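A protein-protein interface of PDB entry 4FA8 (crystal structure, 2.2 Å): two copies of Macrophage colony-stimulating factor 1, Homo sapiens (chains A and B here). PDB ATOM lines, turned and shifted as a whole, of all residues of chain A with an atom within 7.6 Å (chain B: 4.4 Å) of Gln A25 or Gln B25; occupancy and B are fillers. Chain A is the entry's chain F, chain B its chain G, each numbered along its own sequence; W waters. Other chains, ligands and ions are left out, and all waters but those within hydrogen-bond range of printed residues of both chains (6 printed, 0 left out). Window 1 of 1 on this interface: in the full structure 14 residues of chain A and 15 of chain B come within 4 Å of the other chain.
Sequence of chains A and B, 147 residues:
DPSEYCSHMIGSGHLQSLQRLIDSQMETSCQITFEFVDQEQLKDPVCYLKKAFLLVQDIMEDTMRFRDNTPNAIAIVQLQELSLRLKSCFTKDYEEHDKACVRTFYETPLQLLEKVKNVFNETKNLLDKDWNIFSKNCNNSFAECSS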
ATOM      1  N   GLN A  19     -35.106  -3.290  21.887  1.00  0.00           N
ATOM      2  CA  GLN A  19     -36.178  -2.982  22.854  1.00  0.00           C
ATOM      3  C   GLN A  19     -35.668  -2.856  24.303  1.00  0.00           C
ATOM      4  O   GLN A  19     -36.194  -2.053  25.089  1.00  0.00           O
ATOM      5  CB  GLN A  19     -37.319  -4.000  22.748  1.00  0.00           C
ATOM      6  CG  GLN A  19     -38.555  -3.645  23.568  1.00  0.00           C
ATOM      7  CD  GLN A  19     -39.156  -2.329  23.124  1.00  0.00           C
ATOM      8  OE1 GLN A  19     -39.479  -2.157  21.945  1.00  0.00           O
ATOM      9  NE2 GLN A  19     -39.269  -1.377  24.050  1.00  0.00           N
ATOM     10  N   ARG A  20     -34.657  -3.659  24.646  1.00  0.00           N
ATOM     11  CA  ARG A  20     -33.991  -3.576  25.940  1.00  0.00           C
ATOM     12  C   ARG A  20     -33.224  -2.267  26.113  1.00  0.00           C
ATOM     13  O   ARG A  20     -33.212  -1.717  27.213  1.00  0.00           O
ATOM     14  CB  ARG A  20     -33.065  -4.775  26.190  1.00  0.00           C
ATOM     15  CG  ARG A  20     -33.767  -6.053  26.611  1.00  0.00           C
ATOM     16  CD  ARG A  20     -32.804  -7.236  26.763  1.00  0.00           C
ATOM     17  NE  ARG A  20     -32.177  -7.635  25.489  1.00  0.00           N
ATOM     18  CZ  ARG A  20     -31.830  -8.879  25.161  1.00  0.00           C
ATOM     19  NH1 ARG A  20     -32.044  -9.882  25.999  1.00  0.00           N
ATOM     20  NH2 ARG A  20     -31.275  -9.125  23.984  1.00  0.00           N
ATOM     21  N   LEU A  21     -32.590  -1.767  25.050  1.00  0.00           N
ATOM     22  CA  LEU A  21     -31.946  -0.448  25.096  1.00  0.00           C
ATOM     23  C   LEU A  21     -32.994   0.590  25.444  1.00  0.00           C
ATOM     24  O   LEU A  21     -32.797   1.411  26.344  1.00  0.00           O
ATOM     25  CB  LEU A  21     -31.318  -0.048  23.753  1.00  0.00           C
ATOM     26  CG  LEU A  21     -30.343  -0.960  23.011  1.00  0.00           C
ATOM     27  CD1 LEU A  21     -30.042  -0.373  21.644  1.00  0.00           C
ATOM     28  CD2 LEU A  21     -29.047  -1.136  23.762  1.00  0.00           C
ATOM     29  N   ILE A  22     -34.103   0.552  24.715  1.00  0.00           N
ATOM     30  CA  ILE A  22     -35.222   1.437  24.982  1.00  0.00           C
ATOM     31  C   ILE A  22     -35.708   1.292  26.427  1.00  0.00           C
ATOM     32  O   ILE A  22     -35.633   2.254  27.163  1.00  0.00           O
ATOM     33  CB  ILE A  22     -36.379   1.254  23.976  1.00  0.00           C
ATOM     34  CG1 ILE A  22     -36.024   1.935  22.654  1.00  0.00           C
ATOM     35  CG2 ILE A  22     -37.673   1.858  24.527  1.00  0.00           C
ATOM     36  CD1 ILE A  22     -36.743   1.370  21.450  1.00  0.00           C
ATOM     37  N   ASP A  23     -36.120   0.091  26.836  1.00  0.00           N
ATOM     38  CA  ASP A  23     -36.793  -0.111  28.148  1.00  0.00           C
ATOM     39  C   ASP A  23     -35.916   0.254  29.340  1.00  0.00           C
ATOM     40  O   ASP A  23     -36.417   0.554  30.438  1.00  0.00           O
ATOM     41  CB  ASP A  23     -37.295  -1.548  28.314  1.00  0.00           C
ATOM     42  CG  ASP A  23     -38.447  -1.886  27.377  1.00  0.00           C
ATOM     43  OD1 ASP A  23     -38.737  -3.088  27.191  1.00  0.00           O
ATOM     44  OD2 ASP A  23     -39.077  -0.962  26.823  1.00  0.00           O
ATOM     45  N   SER A  24     -34.604   0.250  29.125  1.00  0.00           N
ATOM     46  CA  SER A  24     -33.669   0.462  30.214  1.00  0.00           C
ATOM     47  C   SER A  24     -33.263   1.931  30.421  1.00  0.00           C
ATOM     48  O   SER A  24     -32.678   2.264  31.449  1.00  0.00           O
ATOM     49  CB  SER A  24     -32.452  -0.453  30.043  1.00  0.00           C
ATOM     50  OG  SER A  24     -31.738  -0.144  28.837  1.00  0.00           O
ATOM     51  N   GLN A  25     -33.572   2.809  29.462  1.00  0.00           N
ATOM     52  CA  GLN A  25     -33.247   4.244  29.594  1.00  0.00           C
ATOM     53  C   GLN A  25     -34.140   4.960  30.618  1.00  0.00           C
ATOM     54  O   GLN A  25     -35.361   4.867  30.562  1.00  0.00           O
ATOM     55  CB  GLN A  25     -33.318   4.988  28.255  1.00  0.00           C
ATOM     56  CG  GLN A  25     -32.411   4.447  27.152  1.00  0.00           C
ATOM     57  CD  GLN A  25     -30.982   4.208  27.602  1.00  0.00           C
ATOM     58  OE1 GLN A  25     -30.261   5.139  27.941  1.00  0.00           O
ATOM     59  NE2 GLN A  25     -30.566   2.953  27.595  1.00  0.00           N
ATOM     60  N   MET A  26     -33.498   5.678  31.533  1.00  0.00           N
ATOM     61  CA  MET A  26     -34.162   6.560  32.474  1.00  0.00           C
ATOM     62  C   MET A  26     -34.801   7.734  31.730  1.00  0.00           C
ATOM     63  O   MET A  26     -34.236   8.257  30.747  1.00  0.00           O
ATOM     64  CB  MET A  26     -33.133   7.066  33.472  1.00  0.00           C
ATOM     65  CG  MET A  26     -33.657   7.258  34.878  1.00  0.00           C
ATOM     66  SD  MET A  26     -32.339   7.625  36.063  1.00  0.00           S
ATOM     67  CE  MET A  26     -32.023   9.366  35.782  1.00  0.00           C
ATOM     68  N   GLU A  27     -35.981   8.130  32.193  1.00  0.00           N
ATOM     69  CA  GLU A  27     -36.754   9.213  31.584  1.00  0.00           C
ATOM     70  C   GLU A  27     -36.307  10.582  32.087  1.00  0.00           C
ATOM     71  O   GLU A  27     -36.461  10.895  33.280  1.00  0.00           O
ATOM     72  CB  GLU A  27     -38.255   8.992  31.827  1.00  0.00           C
ATOM     73  CG  GLU A  27     -38.827   7.862  30.984  1.00  0.00           C
ATOM     74  CD  GLU A  27     -40.151   7.284  31.471  1.00  0.00           C
ATOM     75  OE1 GLU A  27     -40.787   7.817  32.419  1.00  0.00           O
ATOM     76  OE2 GLU A  27     -40.568   6.269  30.873  1.00  0.00           O
ATOM     77  N   THR A  28     -35.726  11.377  31.183  1.00  0.00           N
ATOM     78  CA  THR A  28     -35.393  12.783  31.447  1.00  0.00           C
ATOM     79  C   THR A  28     -35.990  13.634  30.339  1.00  0.00           C
ATOM     80  O   THR A  28     -36.464  13.096  29.363  1.00  0.00           O
ATOM     81  CB  THR A  28     -33.875  13.019  31.511  1.00  0.00           C
ATOM     82  OG1 THR A  28     -33.308  12.844  30.205  1.00  0.00           O
ATOM     83  CG2 THR A  28     -33.221  12.035  32.466  1.00  0.00           C
ATOM     84  N   ARG A  65     -23.588   5.056  22.814  1.00  0.00           N
ATOM     85  CA  ARG A  65     -22.388   4.641  23.502  1.00  0.00           C
ATOM     86  C   ARG A  65     -22.657   4.111  24.918  1.00  0.00           C
ATOM     87  O   ARG A  65     -23.275   4.781  25.731  1.00  0.00           O
ATOM     88  CB  ARG A  65     -21.440   5.831  23.535  1.00  0.00           C
ATOM     89  CG  ARG A  65     -21.154   6.380  22.140  1.00  0.00           C
ATOM     90  CD  ARG A  65     -20.261   7.603  22.184  1.00  0.00           C
ATOM     91  NE  ARG A  65     -18.936   7.273  22.701  1.00  0.00           N
ATOM     92  CZ  ARG A  65     -18.032   6.552  22.040  1.00  0.00           C
ATOM     93  NH1 ARG A  65     -16.858   6.295  22.597  1.00  0.00           N
ATOM     94  NH2 ARG A  65     -18.307   6.065  20.834  1.00  0.00           N
ATOM     95  N   PHE A  66     -22.180   2.899  25.188  1.00  0.00           N
ATOM     96  CA  PHE A  66     -22.328   2.264  26.483  1.00  0.00           C
ATOM     97  C   PHE A  66     -20.977   1.788  26.985  1.00  0.00           C
ATOM     98  O   PHE A  66     -20.048   1.592  26.196  1.00  0.00           O
ATOM     99  CB  PHE A  66     -23.298   1.092  26.388  1.00  0.00           C
ATOM    100  CG  PHE A  66     -24.678   1.478  25.941  1.00  0.00           C
ATOM    101  CD1 PHE A  66     -25.035   1.403  24.600  1.00  0.00           C
ATOM    102  CD2 PHE A  66     -25.631   1.916  26.865  1.00  0.00           C
ATOM    103  CE1 PHE A  66     -26.307   1.762  24.180  1.00  0.00           C
ATOM    104  CE2 PHE A  66     -26.905   2.266  26.451  1.00  0.00           C
ATOM    105  CZ  PHE A  66     -27.251   2.184  25.110  1.00  0.00           C
ATOM    106  N   ARG A  67     -20.870   1.627  28.300  1.00  0.00           N
ATOM    107  CA  ARG A  67     -19.683   1.087  28.956  1.00  0.00           C
ATOM    108  C   ARG A  67     -19.428  -0.327  28.454  1.00  0.00           C
ATOM    109  O   ARG A  67     -20.375  -1.072  28.210  1.00  0.00           O
ATOM    110  CB  ARG A  67     -19.915   1.082  30.467  1.00  0.00           C
ATOM    111  CG  ARG A  67     -18.681   0.961  31.347  1.00  0.00           C
ATOM    112  CD  ARG A  67     -19.031   1.140  32.824  1.00  0.00           C
ATOM    113  NE  ARG A  67     -19.737   2.405  33.065  1.00  0.00           N
ATOM    114  CZ  ARG A  67     -19.802   3.040  34.240  1.00  0.00           C
ATOM    115  NH1 ARG A  67     -19.197   2.547  35.315  1.00  0.00           N
ATOM    116  NH2 ARG A  67     -20.474   4.182  34.340  1.00  0.00           N
ATOM    117  N   THR A  70     -20.908  -4.378  28.918  1.00  0.00           N
ATOM    118  CA  THR A  70     -22.205  -4.138  29.471  1.00  0.00           C
ATOM    119  C   THR A  70     -23.191  -4.739  28.445  1.00  0.00           C
ATOM    120  O   THR A  70     -22.873  -4.799  27.243  1.00  0.00           O
ATOM    121  CB  THR A  70     -22.346  -2.617  29.676  1.00  0.00           C
ATOM    122  OG1 THR A  70     -22.659  -2.330  31.042  1.00  0.00           O
ATOM    123  CG2 THR A  70     -23.341  -1.971  28.735  1.00  0.00           C
ATOM    124  N   ASN A  72     -25.943  -3.621  27.052  1.00  0.00           N
ATOM    125  CA  ASN A  72     -26.281  -2.698  25.969  1.00  0.00           C
ATOM    126  C   ASN A  72     -25.094  -2.432  25.017  1.00  0.00           C
ATOM    127  O   ASN A  72     -25.281  -2.293  23.808  1.00  0.00           O
ATOM    128  CB  ASN A  72     -26.916  -1.409  26.505  1.00  0.00           C
ATOM    129  CG  ASN A  72     -28.314  -1.634  27.096  1.00  0.00           C
ATOM    130  OD1 ASN A  72     -28.928  -2.682  26.897  1.00  0.00           O
ATOM    131  ND2 ASN A  72     -28.820  -0.644  27.822  1.00  0.00           N
ATOM    132  N   PRO A 109     -33.067  10.993  23.755  1.00  0.00           N
ATOM    133  CA  PRO A 109     -32.418   9.708  23.522  1.00  0.00           C
ATOM    134  C   PRO A 109     -33.402   8.556  23.261  1.00  0.00           C
ATOM    135  O   PRO A 109     -33.183   7.772  22.329  1.00  0.00           O
ATOM    136  CB  PRO A 109     -31.626   9.491  24.809  1.00  0.00           C
ATOM    137  CG  PRO A 109     -31.261  10.869  25.238  1.00  0.00           C
ATOM    138  CD  PRO A 109     -32.472  11.699  24.908  1.00  0.00           C
ATOM    139  N   LEU A 110     -34.478   8.453  24.051  1.00  0.00           N
ATOM    140  CA  LEU A 110     -35.537   7.482  23.779  1.00  0.00           C
ATOM    141  C   LEU A 110     -36.109   7.608  22.364  1.00  0.00           C
ATOM    142  O   LEU A 110     -36.371   6.606  21.707  1.00  0.00           O
ATOM    143  CB  LEU A 110     -36.663   7.570  24.826  1.00  0.00           C
ATOM    144  CG  LEU A 110     -36.439   6.767  26.121  1.00  0.00           C
ATOM    145  CD1 LEU A 110     -37.342   7.213  27.261  1.00  0.00           C
ATOM    146  CD2 LEU A 110     -36.585   5.273  25.868  1.00  0.00           C
ATOM    147  N   LEU A 113     -33.481   6.198  19.839  1.00  0.00           N
ATOM    148  CA  LEU A 113     -33.547   4.751  19.922  1.00  0.00           C
ATOM    149  C   LEU A 113     -34.719   4.181  19.146  1.00  0.00           C
ATOM    150  O   LEU A 113     -34.586   3.168  18.453  1.00  0.00           O
ATOM    151  CB  LEU A 113     -33.608   4.332  21.388  1.00  0.00           C
ATOM    152  CG  LEU A 113     -32.299   3.863  22.025  1.00  0.00           C
ATOM    153  CD1 LEU A 113     -31.062   4.075  21.145  1.00  0.00           C
ATOM    154  CD2 LEU A 113     -32.110   4.478  23.392  1.00  0.00           C
ATOM    155  N   LEU B  21     -29.083  -0.219  36.498  1.00  0.00           N
ATOM    156  CA  LEU B  21     -29.494   1.117  36.055  1.00  0.00           C
ATOM    157  C   LEU B  21     -28.317   1.871  35.435  1.00  0.00           C
ATOM    158  O   LEU B  21     -28.413   2.393  34.320  1.00  0.00           O
ATOM    159  CB  LEU B  21     -30.035   1.945  37.224  1.00  0.00           C
ATOM    160  CG  LEU B  21     -31.090   1.338  38.155  1.00  0.00           C
ATOM    161  CD1 LEU B  21     -31.473   2.357  39.221  1.00  0.00           C
ATOM    162  CD2 LEU B  21     -32.313   0.935  37.358  1.00  0.00           C
ATOM    163  N   ILE B  22     -27.222   1.923  36.185  1.00  0.00           N
ATOM    164  CA  ILE B  22     -26.014   2.595  35.780  1.00  0.00           C
ATOM    165  C   ILE B  22     -25.539   1.982  34.458  1.00  0.00           C
ATOM    166  O   ILE B  22     -25.425   2.682  33.476  1.00  0.00           O
ATOM    167  CB  ILE B  22     -24.935   2.511  36.888  1.00  0.00           C
ATOM    168  CG1 ILE B  22     -25.363   3.355  38.105  1.00  0.00           C
ATOM    169  CG2 ILE B  22     -23.588   2.977  36.369  1.00  0.00           C
ATOM    170  CD1 ILE B  22     -24.634   3.032  39.389  1.00  0.00           C
ATOM    171  N   ASP B  23     -25.341   0.669  34.441  1.00  0.00           N
ATOM    172  CA  ASP B  23     -24.800  -0.042  33.280  1.00  0.00           C
ATOM    173  C   ASP B  23     -25.649   0.100  32.018  1.00  0.00           C
ATOM    174  O   ASP B  23     -25.130  -0.002  30.908  1.00  0.00           O
ATOM    175  CB  ASP B  23     -24.572  -1.531  33.610  1.00  0.00           C
ATOM    176  CG  ASP B  23     -23.333  -1.767  34.485  1.00  0.00           C
ATOM    177  OD1 ASP B  23     -23.078  -2.932  34.864  1.00  0.00           O
ATOM    178  OD2 ASP B  23     -22.609  -0.800  34.792  1.00  0.00           O
ATOM    179  N   SER B  24     -26.945   0.349  32.178  1.00  0.00           N
ATOM    180  CA  SER B  24     -27.834   0.402  31.017  1.00  0.00           C
ATOM    181  C   SER B  24     -28.002   1.785  30.369  1.00  0.00           C
ATOM    182  O   SER B  24     -28.421   1.869  29.208  1.00  0.00           O
ATOM    183  CB  SER B  24     -29.192  -0.243  31.334  1.00  0.00           C
ATOM    184  OG  SER B  24     -29.726   0.243  32.554  1.00  0.00           O
ATOM    185  N   GLN B  25     -27.658   2.855  31.094  1.00  0.00           N
ATOM    186  CA  GLN B  25     -27.798   4.218  30.584  1.00  0.00           C
ATOM    187  C   GLN B  25     -26.827   4.547  29.442  1.00  0.00           C
ATOM    188  O   GLN B  25     -25.638   4.277  29.546  1.00  0.00           O
ATOM    189  CB  GLN B  25     -27.612   5.235  31.706  1.00  0.00           C
ATOM    190  CG  GLN B  25     -28.635   5.128  32.834  1.00  0.00           C
ATOM    191  CD  GLN B  25     -29.993   4.763  32.310  1.00  0.00           C
ATOM    192  OE1 GLN B  25     -30.644   5.564  31.661  1.00  0.00           O
ATOM    193  NE2 GLN B  25     -30.407   3.537  32.551  1.00  0.00           N
ATOM    194  N   MET B  26     -27.369   5.121  28.369  1.00  0.00           N
ATOM    195  CA  MET B  26     -26.610   5.735  27.275  1.00  0.00           C
ATOM    196  C   MET B  26     -25.755   6.891  27.763  1.00  0.00           C
ATOM    197  O   MET B  26     -26.247   7.752  28.490  1.00  0.00           O
ATOM    198  CB  MET B  26     -27.585   6.330  26.262  1.00  0.00           C
ATOM    199  CG  MET B  26     -27.867   5.484  25.041  1.00  0.00           C
ATOM    200  SD  MET B  26     -29.129   6.243  23.996  1.00  0.00           S
ATOM    201  CE  MET B  26     -28.295   7.706  23.390  1.00  0.00           C
ATOM    202  N   GLU B  27     -24.493   6.941  27.345  1.00  0.00           N
ATOM    203  CA  GLU B  27     -23.642   8.077  27.687  1.00  0.00           C
ATOM    204  C   GLU B  27     -24.026   9.324  26.878  1.00  0.00           C
ATOM    205  O   GLU B  27     -24.040   9.294  25.649  1.00  0.00           O
ATOM    206  CB  GLU B  27     -22.166   7.725  27.510  1.00  0.00           C
ATOM    207  CG  GLU B  27     -21.618   6.749  28.545  1.00  0.00           C
ATOM    208  CD  GLU B  27     -20.386   5.979  28.064  1.00  0.00           C
ATOM    209  OE1 GLU B  27     -19.880   6.267  26.961  1.00  0.00           O
ATOM    210  OE2 GLU B  27     -19.915   5.081  28.795  1.00  0.00           O
ATOM    211  N   PHE B  66     -38.754   5.162  34.987  1.00  0.00           N
ATOM    212  CA  PHE B  66     -38.699   4.213  33.866  1.00  0.00           C
ATOM    213  C   PHE B  66     -40.123   3.792  33.503  1.00  0.00           C
ATOM    214  O   PHE B  66     -41.012   3.925  34.326  1.00  0.00           O
ATOM    215  CB  PHE B  66     -37.883   2.966  34.257  1.00  0.00           C
ATOM    216  CG  PHE B  66     -36.497   3.272  34.737  1.00  0.00           C
ATOM    217  CD1 PHE B  66     -36.260   3.539  36.082  1.00  0.00           C
ATOM    218  CD2 PHE B  66     -35.423   3.311  33.844  1.00  0.00           C
ATOM    219  CE1 PHE B  66     -34.980   3.831  36.533  1.00  0.00           C
ATOM    220  CE2 PHE B  66     -34.140   3.594  34.293  1.00  0.00           C
ATOM    221  CZ  PHE B  66     -33.915   3.855  35.635  1.00  0.00           C
ATOM    222  N   ASN B  72     -36.018  -2.055  35.065  1.00  0.00           N
ATOM    223  CA  ASN B  72     -35.580  -0.944  35.918  1.00  0.00           C
ATOM    224  C   ASN B  72     -36.722  -0.289  36.717  1.00  0.00           C
ATOM    225  O   ASN B  72     -36.512   0.160  37.847  1.00  0.00           O
ATOM    226  CB  ASN B  72     -34.829   0.095  35.102  1.00  0.00           C
ATOM    227  CG  ASN B  72     -33.518  -0.442  34.489  1.00  0.00           C
ATOM    228  OD1 ASN B  72     -33.010  -1.510  34.847  1.00  0.00           O
ATOM    229  ND2 ASN B  72     -32.968   0.325  33.580  1.00  0.00           N
ATOM    230  N   LEU B 110     -26.267   9.618  34.832  1.00  0.00           N
ATOM    231  CA  LEU B 110     -25.274   8.649  35.278  1.00  0.00           C
ATOM    232  C   LEU B 110     -24.599   9.066  36.580  1.00  0.00           C
ATOM    233  O   LEU B 110     -24.290   8.219  37.420  1.00  0.00           O
ATOM    234  CB  LEU B 110     -24.213   8.370  34.186  1.00  0.00           C
ATOM    235  CG  LEU B 110     -24.557   7.192  33.263  1.00  0.00           C
ATOM    236  CD1 LEU B 110     -23.583   7.061  32.098  1.00  0.00           C
ATOM    237  CD2 LEU B 110     -24.613   5.883  34.046  1.00  0.00           C
ATOM    238  N   LEU B 113     -26.984   8.616  39.378  1.00  0.00           N
ATOM    239  CA  LEU B 113     -27.084   7.191  39.629  1.00  0.00           C
ATOM    240  C   LEU B 113     -25.886   6.685  40.421  1.00  0.00           C
ATOM    241  O   LEU B 113     -26.053   5.868  41.319  1.00  0.00           O
ATOM    242  CB  LEU B 113     -27.253   6.443  38.305  1.00  0.00           C
ATOM    243  CG  LEU B 113     -28.630   5.909  37.855  1.00  0.00           C
ATOM    244  CD1 LEU B 113     -29.840   6.486  38.586  1.00  0.00           C
ATOM    245  CD2 LEU B 113     -28.782   6.052  36.349  1.00  0.00           C
HETATM  246  O   HOH W   1     -42.716   6.876  34.701  1.00  0.00           O
HETATM  247  O   HOH W   2     -22.966   1.554  29.733  1.00  0.00           O
HETATM  248  O   HOH W   3     -18.426   7.669  25.398  1.00  0.00           O
HETATM  249  O   HOH W   4     -26.307  -2.281  29.609  1.00  0.00           O
HETATM  250  O   HOH W   5     -24.370   7.501  23.571  1.00  0.00           O
HETATM  251  O   HOH W   6     -35.304  -1.744  32.121  1.00  0.00           O
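Printed residues of chain A within 4 Å of Gln B25: Ser A24, Gln A25, Met A26 and Phe A66. Of the printed residues of chain A, Leu B113 touches Met A26. Of the printed residues of chain A, Asp B23 touches Thr A70 (3.3 Å). Of the printed residues of chain A, Met B26 touches Gln A25 (2.9 Å), Arg A65 (3.8 Å), Phe A66 (3.4 Å) and Leu A113 (3.5 Å). Arg A20 touches none of the printed residues of chain B. The nearest printed residue of chain B that does not touch Gln A25 is Asn B72 (4.8 Å). The nearest residue of chain A that does not touch Gln B25 is Arg A65 (4.5 Å). The nearest printed residue of chain A that does not touch Leu B113 is Ser A24 (7.3 Å).
The side-chain amide oxygen of Gln A25 is in hydrogen-bond range of the backbone NH of Met B26 (2.9 Å). The backbone carbonyl oxygen (O) of Ser A24 is in hydrogen-bond range of the side-chain amide nitrogen (ND2) of Asn B72 (2.9 Å). N of Met A26 lies within hydrogen-bond range of OE1 of Gln B25, 2.9 Å away. The backbone carbonyl oxygen of Ser B24 sits at hydrogen-bond distance from the side-chain amide nitrogen of Asn A72, 2.9 Å away. N of Glu B27 lies within hydrogen-bond range of O of Arg A65 (3.0 Å). The backbone carbonyl oxygen (O) of Ser B24 lies within hydrogen-bond range of the side-chain amide nitrogen (NE2) of Gln A25, 2.9 Å away. O of Ser A24 is in hydrogen-bond range of NE2 of Gln B25 (2.8 Å). The side-chain hydroxyl (OG1) of Thr A70 lies close to the backbone carbonyl oxygen (O) of Asp B23, 3.4 Å away.
ND2 of Asn B72 lies within hydrogen-bond range of OG of Ser B24 (3.4 Å). The side-chain hydroxyl of Ser A24 is in hydrogen-bond range of the backbone carbonyl oxygen of Leu A21 (3.1 Å). The backbone carbonyl oxygen (O) of Leu B21 is in hydrogen-bond range of the side-chain amide nitrogen (NE2) of Gln B25 (2.9 Å). O of Leu A21 is in hydrogen-bond range of NE2 of Gln A25 (3.0 Å). OG of Ser A24 sits at hydrogen-bond distance from O of Arg A20 (2.7 Å). The side-chain hydroxyl of Ser A24 is in hydrogen-bond range of the side-chain amide nitrogen of Asn A72 (3.1 Å).
Water W2 bridges N of Arg A67 (2.5 Å) and O of Asp B23 (2.9 Å). Water W3 bridges the side-chain carboxylate (OE1) of Glu B27 (2.6 Å) and the guanidinium group (NE) of Arg A65 (2.8 Å). Water W5 lies within hydrogen-bond range of N of Arg A65 (2.7 Å) and O of Glu B27 (2.8 Å). Water W4 bridges O of Asp B23 and N of Asn A72. Water W6 lies within hydrogen-bond range of N of Asn B72 (3.0 Å) and O of Asp A23 (3.1 Å). Water W1 bridges the side-chain carboxylate (OE1) of Glu A27 (3.1 Å) and the backbone carbonyl oxygen (O) of Phe B66 (3.4 Å).
Ser A24 touches Phe B66, and with the chains exchanged Phe A66 touches Ser B24. Ser A24 touches Asn B72, and with the chains exchanged Asn A72 touches Ser B24. Gln A25 touches Met B26, and with the chains exchanged Met A26 touches Gln B25. Glu A27 touches Phe B66, and with the chains exchanged Phe A66 touches Glu B27. Of the 23 pairs that touch across the chains among the printed residues, 18 have their exchanged pair printed and touching as well.
Of the 18 printed residues of chain A, 10 touch a printed residue of chain B. Printed residues of chain A that touch a printed residue of chain B: Ser A24, Gln A25, Met A26, Glu A27, Arg A65, Phe A66, Arg A67, Thr A70, Asn A72 and Leu A113. Hydrophobic or aromatic side chains of chain B that line the printed part of chain A: Ile B22, Met B26, Phe B66 and Leu B113. Among the printed residues, 23 pairs touch across the chains. Among the printed residues, no Asp or Glu carboxylate lies within 4 Å of a Lys or Arg side-chain nitrogen of the other chain.
Ser A24 touches Ser B24 (CB to CB, 3.5 Å). Gln A25 touches Gln B25. CD2 of Phe B66 touches O of Gln A25, at 3.6 Å. CE2 of Phe B66 touches CA of Met A26 (3.5 Å). Leu B113 touches Met A26 (CD1 to SD, 3.7 Å). Glu A27 touches Phe B66. O of Ser B24 touches CE2 of Phe A66, 3.2 Å away. C of Phe A66 touches OE2 of Glu B27, at 3.9 Å. CG2 of Ile B22 touches NH2 of Arg A67, at 3.9 Å. Arg A67 touches Glu B27 (N to OE2, 3.6 Å).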
